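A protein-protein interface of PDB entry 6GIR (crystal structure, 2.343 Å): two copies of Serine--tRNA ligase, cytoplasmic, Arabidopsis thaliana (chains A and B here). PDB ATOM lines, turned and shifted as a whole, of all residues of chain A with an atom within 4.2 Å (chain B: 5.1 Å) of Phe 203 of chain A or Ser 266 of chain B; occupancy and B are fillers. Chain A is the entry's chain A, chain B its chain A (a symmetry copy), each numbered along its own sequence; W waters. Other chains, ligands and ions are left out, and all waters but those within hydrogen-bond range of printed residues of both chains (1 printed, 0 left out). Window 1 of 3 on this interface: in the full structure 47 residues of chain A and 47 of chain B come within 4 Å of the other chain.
Phe 203 of chain A touches Ser 266 of chain B, and with the chains exchanged Ser 266 of chain A touches Phe 203 of chain B.
Phe 203 of chain A touches Phe 268 of chain B, and with the chains exchanged Phe 268 of chain A touches Phe 203 of chain B.
Of the 8 pairs that touch across the chains among the printed residues, 4 have their exchanged pair printed and touching as well.
Among the printed residues, merely in contact across the chains: Ser 266 of chain A with Phe 203 of chain B (3.4 Å), Phe 203 of chain A with Ser 266 of chain B (3.4 Å), Gln 200 of chain A with Glu 289 of chain B (3.5 Å), Pro 202 of chain A with Gln 287 of chain B (3.6 Å), Phe 204 of chain A with Phe 268 of chain B (3.9 Å), Phe 268 of chain A with Phe 203 of chain B (3.9 Å) and Phe 203 of chain A with Phe 268 of chain B (3.9 Å).
The backbone NH (N) of Phe 203 of chain A sits close to the side-chain amide nitrogen (NE2) of Gln 287 of chain B (3.0 Å).
N of Ile 236 of chain A lies within hydrogen-bond range of O of Phe 203 of chain A (3.2 Å).
The backbone carbonyl oxygen (O) of Ile 236 of chain A sits at hydrogen-bond distance from the backbone NH (N) of Phe 268 of chain A (3.0 Å).
The backbone NH of Ile 236 of chain B is in hydrogen-bond range of the backbone carbonyl oxygen of Phe 203 of chain B, 3.2 Å away.
The backbone carbonyl oxygen (O) of Ile 236 of chain B is in hydrogen-bond range of the backbone NH (N) of Phe 268 of chain B, 3.0 Å away.
OG of Ser 266 of chain B is in hydrogen-bond range of OE2 of Glu 289 of chain B, 3.1 Å away.
Phe 203 of chain A touches three residues of chain B.
Of the printed residues of chain B, Phe 204 of chain A touches Phe 268.
Of the printed residues of chain B, Ser 266 of chain A touches Phe 203.
Printed residues of chain B within 4 Å of Phe 268 of chain A: Phe 203 (3.9 Å).
Ser 265 of chain B touches none of the printed residues of chain A.
The nearest residue of chain B that does not touch Phe 203 of chain A is Phe 203 of chain B (4.3 Å).
The nearest printed residue of chain A that does not touch Ser 266 of chain B is Ser 266 of chain A (5.1 Å).
The nearest printed residue of chain A that does not touch Glu 289 of chain B is Phe 203 of chain A (4.7 Å).
Water W1 bridges the side-chain carboxylate of Glu 289 of chain B (3.1 Å) and the side-chain amide nitrogen of Gln 200 of chain A (3.3 Å).
Hydrophobic or aromatic side chains of chain A within 4 Å of the printed part of chain B: Phe 203, Phe 204 and Phe 268.
Of the 10 printed residues of chain B, 5 touch a printed residue of chain A.
Printed residues of chain B that touch a printed residue of chain A: Phe 203, Ser 266, Phe 268, Gln 287 and Glu 289.
Hydrophobic or aromatic side chains of chain B that line the printed part of chain A: Phe 203 and Phe 268.
Along chain B the printed residues that touch a printed residue of chain A span positions 203 to 289.
Among the printed residues, 8 pairs touch across the chains.
Among the printed residues, no Asp or Glu carboxylate lies within 4 Å of a Lys or Arg side-chain nitrogen of the other chain.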
ATOM      1  N   GLN A 200       3.157 -14.826  -1.324  1.00  0.00           N
ATOM      2  CA  GLN A 200       2.953 -15.799  -2.369  1.00  0.00           C
ATOM      3  C   GLN A 200       2.512 -17.114  -1.729  1.00  0.00           C
ATOM      4  O   GLN A 200       3.270 -17.721  -0.970  1.00  0.00           O
ATOM      5  CB  GLN A 200       4.226 -15.988  -3.186  1.00  0.00           C
ATOM      6  CG  GLN A 200       4.105 -16.991  -4.328  1.00  0.00           C
ATOM      7  CD  GLN A 200       5.346 -17.020  -5.203  1.00  0.00           C
ATOM      8  OE1 GLN A 200       5.853 -15.970  -5.606  1.00  0.00           O
ATOM      9  NE2 GLN A 200       5.837 -18.224  -5.510  1.00  0.00           N
ATOM     10  N   PRO A 201       1.290 -17.569  -2.046  1.00  0.00           N
ATOM     11  CA  PRO A 201       0.801 -18.790  -1.463  1.00  0.00           C
ATOM     12  C   PRO A 201       1.310 -20.013  -2.179  1.00  0.00           C
ATOM     13  O   PRO A 201       1.888 -19.903  -3.292  1.00  0.00           O
ATOM     14  CB  PRO A 201      -0.697 -18.693  -1.705  1.00  0.00           C
ATOM     15  CG  PRO A 201      -0.771 -18.064  -3.042  1.00  0.00           C
ATOM     16  CD  PRO A 201       0.379 -17.101  -3.102  1.00  0.00           C
ATOM     17  N   PRO A 202       1.063 -21.183  -1.563  1.00  0.00           N
ATOM     18  CA  PRO A 202       1.202 -22.426  -2.303  1.00  0.00           C
ATOM     19  C   PRO A 202       0.169 -22.384  -3.420  1.00  0.00           C
ATOM     20  O   PRO A 202      -0.882 -21.789  -3.240  1.00  0.00           O
ATOM     21  CB  PRO A 202       0.881 -23.513  -1.270  1.00  0.00           C
ATOM     22  CG  PRO A 202       0.832 -22.849   0.055  1.00  0.00           C
ATOM     23  CD  PRO A 202       0.574 -21.399  -0.185  1.00  0.00           C
ATOM     24  N   PHE A 203       0.500 -22.948  -4.572  1.00  0.00           N
ATOM     25  CA  PHE A 203      -0.413 -23.016  -5.702  1.00  0.00           C
ATOM     26  C   PHE A 203      -1.333 -24.230  -5.604  1.00  0.00           C
ATOM     27  O   PHE A 203      -2.061 -24.511  -6.550  1.00  0.00           O
ATOM     28  CB  PHE A 203       0.336 -23.031  -7.049  1.00  0.00           C
ATOM     29  CG  PHE A 203       1.251 -21.857  -7.287  1.00  0.00           C
ATOM     30  CD1 PHE A 203       1.295 -20.744  -6.449  1.00  0.00           C
ATOM     31  CD2 PHE A 203       2.055 -21.853  -8.402  1.00  0.00           C
ATOM     32  CE1 PHE A 203       2.161 -19.702  -6.698  1.00  0.00           C
ATOM     33  CE2 PHE A 203       2.916 -20.800  -8.664  1.00  0.00           C
ATOM     34  CZ  PHE A 203       2.975 -19.731  -7.805  1.00  0.00           C
ATOM     35  N   PHE A 204      -1.304 -24.970  -4.491  1.00  0.00           N
ATOM     36  CA  PHE A 204      -2.416 -25.867  -4.199  1.00  0.00           C
ATOM     37  C   PHE A 204      -2.833 -25.923  -2.749  1.00  0.00           C
ATOM     38  O   PHE A 204      -2.040 -25.649  -1.864  1.00  0.00           O
ATOM     39  CB  PHE A 204      -2.222 -27.271  -4.794  1.00  0.00           C
ATOM     40  CG  PHE A 204      -0.859 -27.910  -4.575  1.00  0.00           C
ATOM     41  CD1 PHE A 204      -0.414 -28.245  -3.303  1.00  0.00           C
ATOM     42  CD2 PHE A 204      -0.092 -28.301  -5.672  1.00  0.00           C
ATOM     43  CE1 PHE A 204       0.800 -28.897  -3.123  1.00  0.00           C
ATOM     44  CE2 PHE A 204       1.111 -28.946  -5.510  1.00  0.00           C
ATOM     45  CZ  PHE A 204       1.567 -29.243  -4.230  1.00  0.00           C
ATOM     46  N   LEU A 235      -5.696 -27.169  -7.394  1.00  0.00           N
ATOM     47  CA  LEU A 235      -4.910 -25.997  -7.809  1.00  0.00           C
ATOM     48  C   LEU A 235      -5.759 -24.738  -7.584  1.00  0.00           C
ATOM     49  O   LEU A 235      -6.957 -24.714  -7.895  1.00  0.00           O
ATOM     50  CB  LEU A 235      -4.474 -26.074  -9.282  1.00  0.00           C
ATOM     51  CG  LEU A 235      -3.350 -27.045  -9.644  1.00  0.00           C
ATOM     52  CD1 LEU A 235      -3.088 -27.028 -11.137  1.00  0.00           C
ATOM     53  CD2 LEU A 235      -2.072 -26.704  -8.894  1.00  0.00           C
ATOM     54  N   ILE A 236      -5.136 -23.700  -7.050  1.00  0.00           N
ATOM     55  CA  ILE A 236      -5.836 -22.477  -6.749  1.00  0.00           C
ATOM     56  C   ILE A 236      -6.226 -21.797  -8.069  1.00  0.00           C
ATOM     57  O   ILE A 236      -5.451 -21.839  -9.046  1.00  0.00           O
ATOM     58  CB  ILE A 236      -4.998 -21.530  -5.851  1.00  0.00           C
ATOM     59  CG1 ILE A 236      -3.753 -20.962  -6.581  1.00  0.00           C
ATOM     60  CG2 ILE A 236      -4.593 -22.252  -4.576  1.00  0.00           C
ATOM     61  CD1 ILE A 236      -2.999 -19.904  -5.813  1.00  0.00           C
ATOM     62  N   SER A 265       0.274 -15.095  -7.200  1.00  0.00           N
ATOM     63  CA  SER A 265       0.391 -16.489  -7.537  1.00  0.00           C
ATOM     64  C   SER A 265       0.117 -16.646  -8.997  1.00  0.00           C
ATOM     65  O   SER A 265      -0.351 -15.727  -9.661  1.00  0.00           O
ATOM     66  CB  SER A 265      -0.574 -17.338  -6.713  1.00  0.00           C
ATOM     67  OG  SER A 265      -1.932 -17.143  -7.105  1.00  0.00           O
ATOM     68  N   SER A 266       0.512 -17.805  -9.502  1.00  0.00           N
ATOM     69  CA  SER A 266      -0.047 -18.370 -10.695  1.00  0.00           C
ATOM     70  C   SER A 266      -1.433 -18.894 -10.373  1.00  0.00           C
ATOM     71  O   SER A 266      -1.730 -19.305  -9.234  1.00  0.00           O
ATOM     72  CB  SER A 266       0.821 -19.496 -11.204  1.00  0.00           C
ATOM     73  OG  SER A 266       1.997 -18.952 -11.730  1.00  0.00           O
ATOM     74  N   PHE A 268      -4.956 -21.130 -11.965  1.00  0.00           N
ATOM     75  CA  PHE A 268      -5.284 -22.279 -12.798  1.00  0.00           C
ATOM     76  C   PHE A 268      -6.795 -22.402 -12.878  1.00  0.00           C
ATOM     77  O   PHE A 268      -7.435 -22.582 -11.857  1.00  0.00           O
ATOM     78  CB  PHE A 268      -4.670 -23.554 -12.198  1.00  0.00           C
ATOM     79  CG  PHE A 268      -3.177 -23.502 -12.086  1.00  0.00           C
ATOM     80  CD1 PHE A 268      -2.369 -23.903 -13.148  1.00  0.00           C
ATOM     81  CD2 PHE A 268      -2.570 -23.013 -10.922  1.00  0.00           C
ATOM     82  CE1 PHE A 268      -0.973 -23.844 -13.043  1.00  0.00           C
ATOM     83  CE2 PHE A 268      -1.180 -22.944 -10.818  1.00  0.00           C
ATOM     84  CZ  PHE A 268      -0.385 -23.349 -11.886  1.00  0.00           C
ATOM     85  N   PHE B 203       2.966 -24.951 -16.607  1.00  0.00           N
ATOM     86  CA  PHE B 203       3.368 -25.724 -15.442  1.00  0.00           C
ATOM     87  C   PHE B 203       2.710 -27.101 -15.432  1.00  0.00           C
ATOM     88  O   PHE B 203       2.830 -27.818 -14.444  1.00  0.00           O
ATOM     89  CB  PHE B 203       3.060 -24.985 -14.125  1.00  0.00           C
ATOM     90  CG  PHE B 203       3.690 -23.622 -13.993  1.00  0.00           C
ATOM     91  CD1 PHE B 203       4.626 -23.124 -14.898  1.00  0.00           C
ATOM     92  CD2 PHE B 203       3.364 -22.838 -12.910  1.00  0.00           C
ATOM     93  CE1 PHE B 203       5.161 -21.865 -14.745  1.00  0.00           C
ATOM     94  CE2 PHE B 203       3.913 -21.577 -12.745  1.00  0.00           C
ATOM     95  CZ  PHE B 203       4.802 -21.088 -13.669  1.00  0.00           C
ATOM     96  N   ILE B 236       4.982 -30.145 -13.880  1.00  0.00           N
ATOM     97  CA  ILE B 236       6.378 -30.226 -14.230  1.00  0.00           C
ATOM     98  C   ILE B 236       7.210 -30.181 -12.939  1.00  0.00           C
ATOM     99  O   ILE B 236       6.852 -29.452 -11.991  1.00  0.00           O
ATOM    100  CB  ILE B 236       6.799 -29.104 -15.214  1.00  0.00           C
ATOM    101  CG1 ILE B 236       6.758 -27.695 -14.566  1.00  0.00           C
ATOM    102  CG2 ILE B 236       5.925 -29.152 -16.457  1.00  0.00           C
ATOM    103  CD1 ILE B 236       7.322 -26.588 -15.424  1.00  0.00           C
ATOM    104  N   TYR B 264      12.071 -20.516 -17.181  1.00  0.00           N
ATOM    105  CA  TYR B 264      11.599 -20.082 -15.874  1.00  0.00           C
ATOM    106  C   TYR B 264      10.235 -20.720 -15.583  1.00  0.00           C
ATOM    107  O   TYR B 264       9.290 -20.584 -16.353  1.00  0.00           O
ATOM    108  CB  TYR B 264      11.494 -18.551 -15.769  1.00  0.00           C
ATOM    109  CG  TYR B 264      10.696 -18.105 -14.564  1.00  0.00           C
ATOM    110  CD1 TYR B 264      11.081 -18.471 -13.276  1.00  0.00           C
ATOM    111  CD2 TYR B 264       9.520 -17.377 -14.702  1.00  0.00           C
ATOM    112  CE1 TYR B 264      10.334 -18.101 -12.159  1.00  0.00           C
ATOM    113  CE2 TYR B 264       8.772 -16.999 -13.582  1.00  0.00           C
ATOM    114  CZ  TYR B 264       9.189 -17.376 -12.322  1.00  0.00           C
ATOM    115  OH  TYR B 264       8.465 -17.033 -11.218  1.00  0.00           O
ATOM    116  N   SER B 265      10.135 -21.401 -14.454  1.00  0.00           N
ATOM    117  CA  SER B 265       8.857 -21.914 -14.038  1.00  0.00           C
ATOM    118  C   SER B 265       8.898 -22.141 -12.561  1.00  0.00           C
ATOM    119  O   SER B 265       9.953 -22.095 -11.938  1.00  0.00           O
ATOM    120  CB  SER B 265       8.517 -23.210 -14.772  1.00  0.00           C
ATOM    121  OG  SER B 265       9.329 -24.301 -14.343  1.00  0.00           O
ATOM    122  N   SER B 266       7.706 -22.290 -12.002  1.00  0.00           N
ATOM    123  CA  SER B 266       7.506 -22.972 -10.757  1.00  0.00           C
ATOM    124  C   SER B 266       7.667 -24.461 -10.996  1.00  0.00           C
ATOM    125  O   SER B 266       7.396 -24.981 -12.095  1.00  0.00           O
ATOM    126  CB  SER B 266       6.127 -22.685 -10.213  1.00  0.00           C
ATOM    127  OG  SER B 266       6.089 -21.361  -9.765  1.00  0.00           O
ATOM    128  N   CYS B 267       8.110 -25.139  -9.945  1.00  0.00           N
ATOM    129  CA  CYS B 267       8.428 -26.566 -10.000  1.00  0.00           C
ATOM    130  C   CYS B 267       7.705 -27.262  -8.902  1.00  0.00           C
ATOM    131  O   CYS B 267       7.440 -26.667  -7.870  1.00  0.00           O
ATOM    132  CB  CYS B 267       9.923 -26.743  -9.853  1.00  0.00           C
ATOM    133  SG  CYS B 267      10.691 -25.966 -11.284  1.00  0.00           S
ATOM    134  N   PHE B 268       7.362 -28.512  -9.141  1.00  0.00           N
ATOM    135  CA  PHE B 268       6.524 -29.277  -8.228  1.00  0.00           C
ATOM    136  C   PHE B 268       7.112 -30.670  -8.085  1.00  0.00           C
ATOM    137  O   PHE B 268       7.209 -31.381  -9.069  1.00  0.00           O
ATOM    138  CB  PHE B 268       5.088 -29.352  -8.772  1.00  0.00           C
ATOM    139  CG  PHE B 268       4.443 -28.011  -8.942  1.00  0.00           C
ATOM    140  CD1 PHE B 268       3.756 -27.413  -7.888  1.00  0.00           C
ATOM    141  CD2 PHE B 268       4.555 -27.319 -10.156  1.00  0.00           C
ATOM    142  CE1 PHE B 268       3.162 -26.153  -8.048  1.00  0.00           C
ATOM    143  CE2 PHE B 268       3.973 -26.061 -10.314  1.00  0.00           C
ATOM    144  CZ  PHE B 268       3.289 -25.476  -9.254  1.00  0.00           C
ATOM    145  N   GLN B 287       7.235 -27.358  -3.741  1.00  0.00           N
ATOM    146  CA  GLN B 287       7.021 -26.329  -4.763  1.00  0.00           C
ATOM    147  C   GLN B 287       8.056 -25.235  -4.632  1.00  0.00           C
ATOM    148  O   GLN B 287       8.277 -24.671  -3.552  1.00  0.00           O
ATOM    149  CB  GLN B 287       5.636 -25.722  -4.623  1.00  0.00           C
ATOM    150  CG  GLN B 287       5.309 -24.702  -5.708  1.00  0.00           C
ATOM    151  CD  GLN B 287       4.139 -23.798  -5.350  1.00  0.00           C
ATOM    152  OE1 GLN B 287       4.172 -22.601  -5.620  1.00  0.00           O
ATOM    153  NE2 GLN B 287       3.119 -24.361  -4.720  1.00  0.00           N
ATOM    154  N   PHE B 288       8.664 -24.897  -5.748  1.00  0.00           N
ATOM    155  CA  PHE B 288       9.754 -23.932  -5.751  1.00  0.00           C
ATOM    156  C   PHE B 288       9.927 -23.369  -7.159  1.00  0.00           C
ATOM    157  O   PHE B 288       9.374 -23.900  -8.129  1.00  0.00           O
ATOM    158  CB  PHE B 288      11.043 -24.591  -5.228  1.00  0.00           C
ATOM    159  CG  PHE B 288      11.419 -25.846  -5.967  1.00  0.00           C
ATOM    160  CD1 PHE B 288      10.765 -27.048  -5.699  1.00  0.00           C
ATOM    161  CD2 PHE B 288      12.388 -25.816  -6.945  1.00  0.00           C
ATOM    162  CE1 PHE B 288      11.072 -28.195  -6.402  1.00  0.00           C
ATOM    163  CE2 PHE B 288      12.714 -26.964  -7.643  1.00  0.00           C
ATOM    164  CZ  PHE B 288      12.059 -28.157  -7.374  1.00  0.00           C
ATOM    165  N   GLU B 289      10.639 -22.254  -7.256  1.00  0.00           N
ATOM    166  CA  GLU B 289      10.886 -21.609  -8.540  1.00  0.00           C
ATOM    167  C   GLU B 289      12.327 -21.935  -8.939  1.00  0.00           C
ATOM    168  O   GLU B 289      13.193 -22.101  -8.092  1.00  0.00           O
ATOM    169  CB  GLU B 289      10.643 -20.103  -8.451  1.00  0.00           C
ATOM    170  CG  GLU B 289       9.173 -19.723  -8.349  1.00  0.00           C
ATOM    171  CD  GLU B 289       8.522 -20.161  -7.033  1.00  0.00           C
ATOM    172  OE1 GLU B 289       9.038 -19.757  -5.963  1.00  0.00           O
ATOM    173  OE2 GLU B 289       7.502 -20.916  -7.054  1.00  0.00           O
HETATM  174  O   HOH W   1       6.886 -21.003  -3.989  1.00  0.00           O
